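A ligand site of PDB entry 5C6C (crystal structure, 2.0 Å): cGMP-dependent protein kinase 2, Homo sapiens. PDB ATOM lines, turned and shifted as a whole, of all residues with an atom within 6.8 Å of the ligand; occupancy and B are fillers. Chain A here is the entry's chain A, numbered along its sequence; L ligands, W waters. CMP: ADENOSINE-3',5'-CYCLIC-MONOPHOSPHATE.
OE1 of Glu 99 sits at hydrogen-bond distance from O2' of the ligand (2.7 Å).
N of Thr 109 is in hydrogen-bond range of O2P of the ligand, at 2.9 Å.
The side-chain hydroxyl (OG1) of Thr 109 is in hydrogen-bond range of an oxygen (O2P) of the ligand, 2.8 Å away.
NH1 of Arg 108 lies within salt-bridge range of O1P of the ligand.
N of Ala 101 lies within hydrogen-bond range of O1P of the ligand, at 3.0 Å.
The backbone NH (N) of Gly 98 lies within hydrogen-bond range of an oxygen (O2') of the ligand, at 3.0 Å.
The side-chain carboxylate (OE2) of Glu 99 sits at hydrogen-bond distance from the side-chain amide nitrogen (ND2) of Asn 32 (2.9 Å).
The backbone carbonyl oxygen of Thr 109 is in hydrogen-bond range of the side-chain amide nitrogen of Gln 83, at 3.0 Å.
O of Gly 98 is in hydrogen-bond range of NH1 of Arg 108 (2.9 Å).
The backbone carbonyl oxygen (O) of His 70 lies within hydrogen-bond range of the guanidinium group (NH2) of Arg 108 (2.8 Å).
The backbone NH (N) of Cys 106 is in hydrogen-bond range of the backbone carbonyl oxygen (O) of Ala 101 (3.5 Å).
The backbone carbonyl oxygen (O) of Ser 89 sits at hydrogen-bond distance from the backbone NH (N) of Val 81.
The backbone carbonyl oxygen of Ile 62 is in hydrogen-bond range of the backbone NH of Val 112, 2.9 Å away.
N of Leu 88 sits at hydrogen-bond distance from O of Val 81 (2.7 Å).
Residues that only touch the ligand: Ile 62 (3.7 Å), Val 81 (3.9 Å), Ser 89 (3.6 Å), Phe 97 (3.5 Å), Leu 100 (3.5 Å), Ala 110 (3.5 Å) and Val 112 (3.9 Å).
Within 4 Å of the ligand: Ile 62, Val 81, Ser 89, Phe 97, Gly 98, Glu 99, Leu 100, Ala 101, Arg 108, Thr 109, Ala 110 and Val 112.
The nearest printed residue that does not touch the ligand is Leu 88 (4.2 Å).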
ATOM      1  N   ASN A  32     -14.865  10.472  -8.245  1.00  0.00           N
ATOM      2  CA  ASN A  32     -14.157  10.564  -9.515  1.00  0.00           C
ATOM      3  C   ASN A  32     -12.804  11.267  -9.361  1.00  0.00           C
ATOM      4  O   ASN A  32     -12.738  12.391  -8.884  1.00  0.00           O
ATOM      5  CB  ASN A  32     -15.002  11.298 -10.541  1.00  0.00           C
ATOM      6  CG  ASN A  32     -14.304  11.400 -11.859  1.00  0.00           C
ATOM      7  OD1 ASN A  32     -13.487  12.294 -12.051  1.00  0.00           O
ATOM      8  ND2 ASN A  32     -14.579  10.446 -12.764  1.00  0.00           N
ATOM      9  N   ILE A  62     -23.001   7.396 -24.982  1.00  0.00           N
ATOM     10  CA  ILE A  62     -21.817   8.056 -25.512  1.00  0.00           C
ATOM     11  C   ILE A  62     -21.314   7.268 -26.711  1.00  0.00           C
ATOM     12  O   ILE A  62     -21.342   6.031 -26.681  1.00  0.00           O
ATOM     13  CB  ILE A  62     -20.690   8.153 -24.445  1.00  0.00           C
ATOM     14  CG1 ILE A  62     -21.132   9.043 -23.270  1.00  0.00           C
ATOM     15  CG2 ILE A  62     -19.424   8.696 -25.091  1.00  0.00           C
ATOM     16  CD1 ILE A  62     -20.185   9.076 -22.090  1.00  0.00           C
ATOM     17  N   LYS A  63     -20.843   7.959 -27.734  1.00  0.00           N
ATOM     18  CA  LYS A  63     -20.218   7.306 -28.897  1.00  0.00           C
ATOM     19  C   LYS A  63     -18.788   7.774 -29.074  1.00  0.00           C
ATOM     20  O   LYS A  63     -18.503   8.981 -29.119  1.00  0.00           O
ATOM     21  CB  LYS A  63     -21.005   7.580 -30.192  1.00  0.00           C
ATOM     22  CG  LYS A  63     -22.430   7.032 -30.139  1.00  0.00           C
ATOM     23  CD  LYS A  63     -23.224   7.375 -31.393  1.00  0.00           C
ATOM     24  CE  LYS A  63     -24.731   7.230 -31.130  1.00  0.00           C
ATOM     25  NZ  LYS A  63     -25.540   7.322 -32.386  1.00  0.00           N
ATOM     26  N   GLN A  64     -17.883   6.815 -29.205  1.00  0.00           N
ATOM     27  CA  GLN A  64     -16.486   7.117 -29.413  1.00  0.00           C
ATOM     28  C   GLN A  64     -16.306   8.051 -30.624  1.00  0.00           C
ATOM     29  O   GLN A  64     -16.994   7.914 -31.640  1.00  0.00           O
ATOM     30  CB  GLN A  64     -15.695   5.820 -29.605  1.00  0.00           C
ATOM     31  CG  GLN A  64     -14.180   6.016 -29.745  1.00  0.00           C
ATOM     32  CD  GLN A  64     -13.450   4.689 -29.755  1.00  0.00           C
ATOM     33  OE1 GLN A  64     -14.068   3.633 -29.649  1.00  0.00           O
ATOM     34  NE2 GLN A  64     -12.137   4.739 -29.919  1.00  0.00           N
ATOM     35  N   GLY A  68     -17.524  15.952 -26.537  1.00  0.00           N
ATOM     36  CA  GLY A  68     -18.143  15.684 -25.243  1.00  0.00           C
ATOM     37  C   GLY A  68     -19.083  16.773 -24.755  1.00  0.00           C
ATOM     38  O   GLY A  68     -18.641  17.810 -24.294  1.00  0.00           O
ATOM     39  N   HIS A  70     -21.757  16.353 -22.534  1.00  0.00           N
ATOM     40  CA  HIS A  70     -22.372  16.060 -21.229  1.00  0.00           C
ATOM     41  C   HIS A  70     -21.481  15.178 -20.378  1.00  0.00           C
ATOM     42  O   HIS A  70     -20.767  14.309 -20.892  1.00  0.00           O
ATOM     43  CB  HIS A  70     -23.701  15.312 -21.352  1.00  0.00           C
ATOM     44  CG  HIS A  70     -24.475  15.611 -22.588  1.00  0.00           C
ATOM     45  ND1 HIS A  70     -25.332  16.690 -22.700  1.00  0.00           N
ATOM     46  CD2 HIS A  70     -24.535  14.959 -23.777  1.00  0.00           C
ATOM     47  CE1 HIS A  70     -25.871  16.693 -23.892  1.00  0.00           C
ATOM     48  NE2 HIS A  70     -25.410  15.653 -24.566  1.00  0.00           N
ATOM     49  N   VAL A  81     -18.752  -0.180 -21.321  1.00  0.00           N
ATOM     50  CA  VAL A  81     -17.868   0.671 -22.088  1.00  0.00           C
ATOM     51  C   VAL A  81     -17.145  -0.167 -23.141  1.00  0.00           C
ATOM     52  O   VAL A  81     -16.646  -1.256 -22.844  1.00  0.00           O
ATOM     53  CB  VAL A  81     -16.804   1.379 -21.184  1.00  0.00           C
ATOM     54  CG1 VAL A  81     -16.010   2.412 -21.997  1.00  0.00           C
ATOM     55  CG2 VAL A  81     -17.473   2.052 -19.988  1.00  0.00           C
ATOM     56  N   GLN A  83     -14.630  -0.145 -26.931  1.00  0.00           N
ATOM     57  CA  GLN A  83     -14.004   0.369 -28.154  1.00  0.00           C
ATOM     58  C   GLN A  83     -14.267  -0.613 -29.284  1.00  0.00           C
ATOM     59  O   GLN A  83     -13.728  -1.725 -29.310  1.00  0.00           O
ATOM     60  CB  GLN A  83     -12.517   0.590 -27.951  1.00  0.00           C
ATOM     61  CG  GLN A  83     -12.270   1.730 -27.015  1.00  0.00           C
ATOM     62  CD  GLN A  83     -10.819   2.018 -26.823  1.00  0.00           C
ATOM     63  OE1 GLN A  83      -9.964   1.155 -27.038  1.00  0.00           O
ATOM     64  NE2 GLN A  83     -10.519   3.223 -26.399  1.00  0.00           N
ATOM     65  N   LEU A  88     -14.521  -2.946 -22.621  1.00  0.00           N
ATOM     66  CA  LEU A  88     -13.534  -2.316 -21.760  1.00  0.00           C
ATOM     67  C   LEU A  88     -13.860  -2.456 -20.279  1.00  0.00           C
ATOM     68  O   LEU A  88     -12.971  -2.736 -19.484  1.00  0.00           O
ATOM     69  CB  LEU A  88     -13.413  -0.816 -22.098  1.00  0.00           C
ATOM     70  CG  LEU A  88     -12.270  -0.431 -23.044  1.00  0.00           C
ATOM     71  CD1 LEU A  88     -12.155  -1.390 -24.207  1.00  0.00           C
ATOM     72  CD2 LEU A  88     -12.410   0.998 -23.520  1.00  0.00           C
ATOM     73  N   SER A  89     -15.126  -2.250 -19.920  1.00  0.00           N
ATOM     74  CA  SER A  89     -15.524  -2.171 -18.517  1.00  0.00           C
ATOM     75  C   SER A  89     -17.048  -2.128 -18.316  1.00  0.00           C
ATOM     76  O   SER A  89     -17.776  -1.658 -19.187  1.00  0.00           O
ATOM     77  CB  SER A  89     -14.902  -0.934 -17.868  1.00  0.00           C
ATOM     78  OG  SER A  89     -15.579  -0.568 -16.682  1.00  0.00           O
ATOM     79  N   SER A  90     -17.496  -2.621 -17.158  1.00  0.00           N
ATOM     80  CA  SER A  90     -18.877  -2.445 -16.690  1.00  0.00           C
ATOM     81  C   SER A  90     -18.943  -1.312 -15.672  1.00  0.00           C
ATOM     82  O   SER A  90     -18.233  -1.346 -14.668  1.00  0.00           O
ATOM     83  CB  SER A  90     -19.411  -3.732 -16.046  1.00  0.00           C
ATOM     84  OG  SER A  90     -19.465  -4.790 -16.977  1.00  0.00           O
ATOM     85  N   ILE A  91     -19.797  -0.325 -15.915  1.00  0.00           N
ATOM     86  CA  ILE A  91     -19.887   0.823 -15.023  1.00  0.00           C
ATOM     87  C   ILE A  91     -20.737   0.540 -13.780  1.00  0.00           C
ATOM     88  O   ILE A  91     -21.927   0.281 -13.899  1.00  0.00           O
ATOM     89  CB  ILE A  91     -20.478   2.024 -15.749  1.00  0.00           C
ATOM     90  CG1 ILE A  91     -19.706   2.272 -17.045  1.00  0.00           C
ATOM     91  CG2 ILE A  91     -20.479   3.252 -14.833  1.00  0.00           C
ATOM     92  CD1 ILE A  91     -20.024   3.627 -17.665  1.00  0.00           C
ATOM     93  N   THR A  96     -19.427   8.325 -11.987  1.00  0.00           N
ATOM     94  CA  THR A  96     -19.365   9.418 -12.946  1.00  0.00           C
ATOM     95  C   THR A  96     -18.671   8.956 -14.223  1.00  0.00           C
ATOM     96  O   THR A  96     -17.619   8.324 -14.162  1.00  0.00           O
ATOM     97  CB  THR A  96     -18.606  10.635 -12.367  1.00  0.00           C
ATOM     98  OG1 THR A  96     -19.232  11.039 -11.149  1.00  0.00           O
ATOM     99  CG2 THR A  96     -18.601  11.813 -13.356  1.00  0.00           C
ATOM    100  N   PHE A  97     -19.247   9.262 -15.374  1.00  0.00           N
ATOM    101  CA  PHE A  97     -18.564   8.931 -16.610  1.00  0.00           C
ATOM    102  C   PHE A  97     -18.836  10.012 -17.661  1.00  0.00           C
ATOM    103  O   PHE A  97     -19.702  10.867 -17.480  1.00  0.00           O
ATOM    104  CB  PHE A  97     -18.997   7.540 -17.131  1.00  0.00           C
ATOM    105  CG  PHE A  97     -20.439   7.481 -17.525  1.00  0.00           C
ATOM    106  CD1 PHE A  97     -21.430   7.313 -16.567  1.00  0.00           C
ATOM    107  CD2 PHE A  97     -20.808   7.569 -18.869  1.00  0.00           C
ATOM    108  CE1 PHE A  97     -22.775   7.247 -16.926  1.00  0.00           C
ATOM    109  CE2 PHE A  97     -22.153   7.503 -19.229  1.00  0.00           C
ATOM    110  CZ  PHE A  97     -23.142   7.353 -18.247  1.00  0.00           C
ATOM    111  N   GLY A  98     -18.075   9.977 -18.753  1.00  0.00           N
ATOM    112  CA  GLY A  98     -18.197  11.002 -19.777  1.00  0.00           C
ATOM    113  C   GLY A  98     -17.482  12.278 -19.380  1.00  0.00           C
ATOM    114  O   GLY A  98     -17.727  13.353 -19.960  1.00  0.00           O
ATOM    115  N   GLU A  99     -16.581  12.170 -18.397  1.00  0.00           N
ATOM    116  CA  GLU A  99     -15.862  13.352 -17.906  1.00  0.00           C
ATOM    117  C   GLU A  99     -14.595  13.695 -18.704  1.00  0.00           C
ATOM    118  O   GLU A  99     -14.192  14.845 -18.749  1.00  0.00           O
ATOM    119  CB  GLU A  99     -15.509  13.165 -16.418  1.00  0.00           C
ATOM    120  CG  GLU A  99     -14.216  12.392 -16.125  1.00  0.00           C
ATOM    121  CD  GLU A  99     -14.320  10.859 -16.239  1.00  0.00           C
ATOM    122  OE1 GLU A  99     -15.111  10.341 -17.063  1.00  0.00           O
ATOM    123  OE2 GLU A  99     -13.595  10.166 -15.498  1.00  0.00           O
ATOM    124  N   LEU A 100     -13.964  12.709 -19.338  1.00  0.00           N
ATOM    125  CA  LEU A 100     -12.699  12.973 -20.024  1.00  0.00           C
ATOM    126  C   LEU A 100     -12.822  14.006 -21.145  1.00  0.00           C
ATOM    127  O   LEU A 100     -12.031  14.950 -21.240  1.00  0.00           O
ATOM    128  CB  LEU A 100     -12.109  11.677 -20.584  1.00  0.00           C
ATOM    129  CG  LEU A 100     -11.731  10.652 -19.518  1.00  0.00           C
ATOM    130  CD1 LEU A 100     -11.223   9.378 -20.160  1.00  0.00           C
ATOM    131  CD2 LEU A 100     -10.671  11.245 -18.588  1.00  0.00           C
ATOM    132  N   ALA A 101     -13.833  13.839 -21.997  1.00  0.00           N
ATOM    133  CA  ALA A 101     -13.951  14.700 -23.162  1.00  0.00           C
ATOM    134  C   ALA A 101     -14.363  16.115 -22.730  1.00  0.00           C
ATOM    135  O   ALA A 101     -14.116  17.077 -23.421  1.00  0.00           O
ATOM    136  CB  ALA A 101     -14.947  14.123 -24.156  1.00  0.00           C
ATOM    137  N   ILE A 102     -15.015  16.217 -21.577  1.00  0.00           N
ATOM    138  CA  ILE A 102     -15.417  17.506 -21.021  1.00  0.00           C
ATOM    139  C   ILE A 102     -14.232  18.274 -20.443  1.00  0.00           C
ATOM    140  O   ILE A 102     -13.984  19.452 -20.771  1.00  0.00           O
ATOM    141  CB  ILE A 102     -16.464  17.332 -19.902  1.00  0.00           C
ATOM    142  CG1 ILE A 102     -17.748  16.700 -20.446  1.00  0.00           C
ATOM    143  CG2 ILE A 102     -16.776  18.675 -19.250  1.00  0.00           C
ATOM    144  CD1 ILE A 102     -18.595  17.658 -21.243  1.00  0.00           C
ATOM    145  N   CYS A 106     -11.454  17.027 -25.632  1.00  0.00           N
ATOM    146  CA  CYS A 106     -11.089  15.966 -26.547  1.00  0.00           C
ATOM    147  C   CYS A 106     -12.327  15.307 -27.102  1.00  0.00           C
ATOM    148  O   CYS A 106     -13.449  15.709 -26.799  1.00  0.00           O
ATOM    149  CB  CYS A 106     -10.199  14.945 -25.847  1.00  0.00           C
ATOM    150  SG  CYS A 106      -8.637  15.644 -25.336  1.00  0.00           S
ATOM    151  N   THR A 107     -12.144  14.292 -27.935  1.00  0.00           N
ATOM    152  CA  THR A 107     -13.275  13.500 -28.406  1.00  0.00           C
ATOM    153  C   THR A 107     -13.527  12.337 -27.445  1.00  0.00           C
ATOM    154  O   THR A 107     -12.624  11.907 -26.703  1.00  0.00           O
ATOM    155  CB  THR A 107     -13.021  12.971 -29.829  1.00  0.00           C
ATOM    156  OG1 THR A 107     -11.746  12.340 -29.865  1.00  0.00           O
ATOM    157  CG2 THR A 107     -13.000  14.126 -30.827  1.00  0.00           C
ATOM    158  N   ARG A 108     -14.754  11.815 -27.433  1.00  0.00           N
ATOM    159  CA  ARG A 108     -15.080  10.671 -26.602  1.00  0.00           C
ATOM    160  C   ARG A 108     -14.053   9.558 -26.844  1.00  0.00           C
ATOM    161  O   ARG A 108     -13.724   9.263 -27.987  1.00  0.00           O
ATOM    162  CB  ARG A 108     -16.502  10.168 -26.882  1.00  0.00           C
ATOM    163  CG  ARG A 108     -17.629  11.235 -26.634  1.00  0.00           C
ATOM    164  CD  ARG A 108     -17.742  11.626 -25.155  1.00  0.00           C
ATOM    165  NE  ARG A 108     -19.053  12.182 -24.830  1.00  0.00           N
ATOM    166  CZ  ARG A 108     -19.376  12.705 -23.640  1.00  0.00           C
ATOM    167  NH1 ARG A 108     -18.491  12.760 -22.647  1.00  0.00           N
ATOM    168  NH2 ARG A 108     -20.597  13.171 -23.461  1.00  0.00           N
ATOM    169  N   THR A 109     -13.524   9.000 -25.758  1.00  0.00           N
ATOM    170  CA  THR A 109     -12.458   8.000 -25.813  1.00  0.00           C
ATOM    171  C   THR A 109     -12.986   6.589 -26.071  1.00  0.00           C
ATOM    172  O   THR A 109     -12.226   5.673 -26.396  1.00  0.00           O
ATOM    173  CB  THR A 109     -11.624   7.954 -24.492  1.00  0.00           C
ATOM    174  OG1 THR A 109     -12.501   7.687 -23.388  1.00  0.00           O
ATOM    175  CG2 THR A 109     -10.886   9.284 -24.238  1.00  0.00           C
ATOM    176  N   ALA A 110     -14.299   6.423 -25.905  1.00  0.00           N
ATOM    177  CA  ALA A 110     -14.949   5.118 -25.983  1.00  0.00           C
ATOM    178  C   ALA A 110     -16.469   5.271 -26.086  1.00  0.00           C
ATOM    179  O   ALA A 110     -16.985   6.351 -25.846  1.00  0.00           O
ATOM    180  CB  ALA A 110     -14.584   4.266 -24.749  1.00  0.00           C
ATOM    181  N   SER A 111     -17.188   4.216 -26.433  1.00  0.00           N
ATOM    182  CA  SER A 111     -18.634   4.283 -26.436  1.00  0.00           C
ATOM    183  C   SER A 111     -19.203   3.726 -25.117  1.00  0.00           C
ATOM    184  O   SER A 111     -18.574   2.895 -24.465  1.00  0.00           O
ATOM    185  CB  SER A 111     -19.204   3.537 -27.653  1.00  0.00           C
ATOM    186  OG  SER A 111     -18.603   4.004 -28.865  1.00  0.00           O
ATOM    187  N   VAL A 112     -20.362   4.194 -24.711  1.00  0.00           N
ATOM    188  CA  VAL A 112     -20.997   3.659 -23.518  1.00  0.00           C
ATOM    189  C   VAL A 112     -22.395   3.234 -23.902  1.00  0.00           C
ATOM    190  O   VAL A 112     -23.167   4.031 -24.383  1.00  0.00           O
ATOM    191  CB  VAL A 112     -21.027   4.682 -22.368  1.00  0.00           C
ATOM    192  CG1 VAL A 112     -21.753   4.122 -21.177  1.00  0.00           C
ATOM    193  CG2 VAL A 112     -19.599   5.079 -21.989  1.00  0.00           C
HETATM  194  P   CMP L   1     -15.312  10.261 -22.287  1.00  0.00           P
HETATM  195  O1P CMP L   1     -15.884  11.658 -22.232  1.00  0.00           O
HETATM  196  O2P CMP L   1     -14.046  10.003 -23.079  1.00  0.00           O
HETATM  197  O5' CMP L   1     -16.385   9.300 -22.993  1.00  0.00           O
HETATM  198  C5' CMP L   1     -16.390   7.890 -22.789  1.00  0.00           C
HETATM  199  C4' CMP L   1     -16.182   7.635 -21.328  1.00  0.00           C
HETATM  200  O4' CMP L   1     -15.971   6.251 -21.020  1.00  0.00           O
HETATM  201  C3' CMP L   1     -14.941   8.300 -20.780  1.00  0.00           C
HETATM  202  O3' CMP L   1     -15.103   9.696 -20.773  1.00  0.00           O
HETATM  203  C2' CMP L   1     -14.775   7.591 -19.448  1.00  0.00           C
HETATM  204  O2' CMP L   1     -15.689   8.098 -18.482  1.00  0.00           O
HETATM  205  C1' CMP L   1     -15.214   6.164 -19.806  1.00  0.00           C
HETATM  206  N9  CMP L   1     -14.071   5.268 -20.039  1.00  0.00           N
HETATM  207  C8  CMP L   1     -13.165   5.330 -21.048  1.00  0.00           C
HETATM  208  N7  CMP L   1     -12.273   4.313 -20.934  1.00  0.00           N
HETATM  209  C5  CMP L   1     -12.628   3.572 -19.858  1.00  0.00           C
HETATM  210  C6  CMP L   1     -12.107   2.363 -19.177  1.00  0.00           C
HETATM  211  N6  CMP L   1     -11.027   1.701 -19.624  1.00  0.00           N
HETATM  212  N1  CMP L   1     -12.775   1.942 -18.086  1.00  0.00           N
HETATM  213  C2  CMP L   1     -13.857   2.592 -17.610  1.00  0.00           C
HETATM  214  N3  CMP L   1     -14.390   3.676 -18.175  1.00  0.00           N
HETATM  215  C4  CMP L   1     -13.811   4.205 -19.283  1.00  0.00           C
HETATM  216  O   HOH W   1     -16.445   4.466 -16.388  1.00  0.00           O
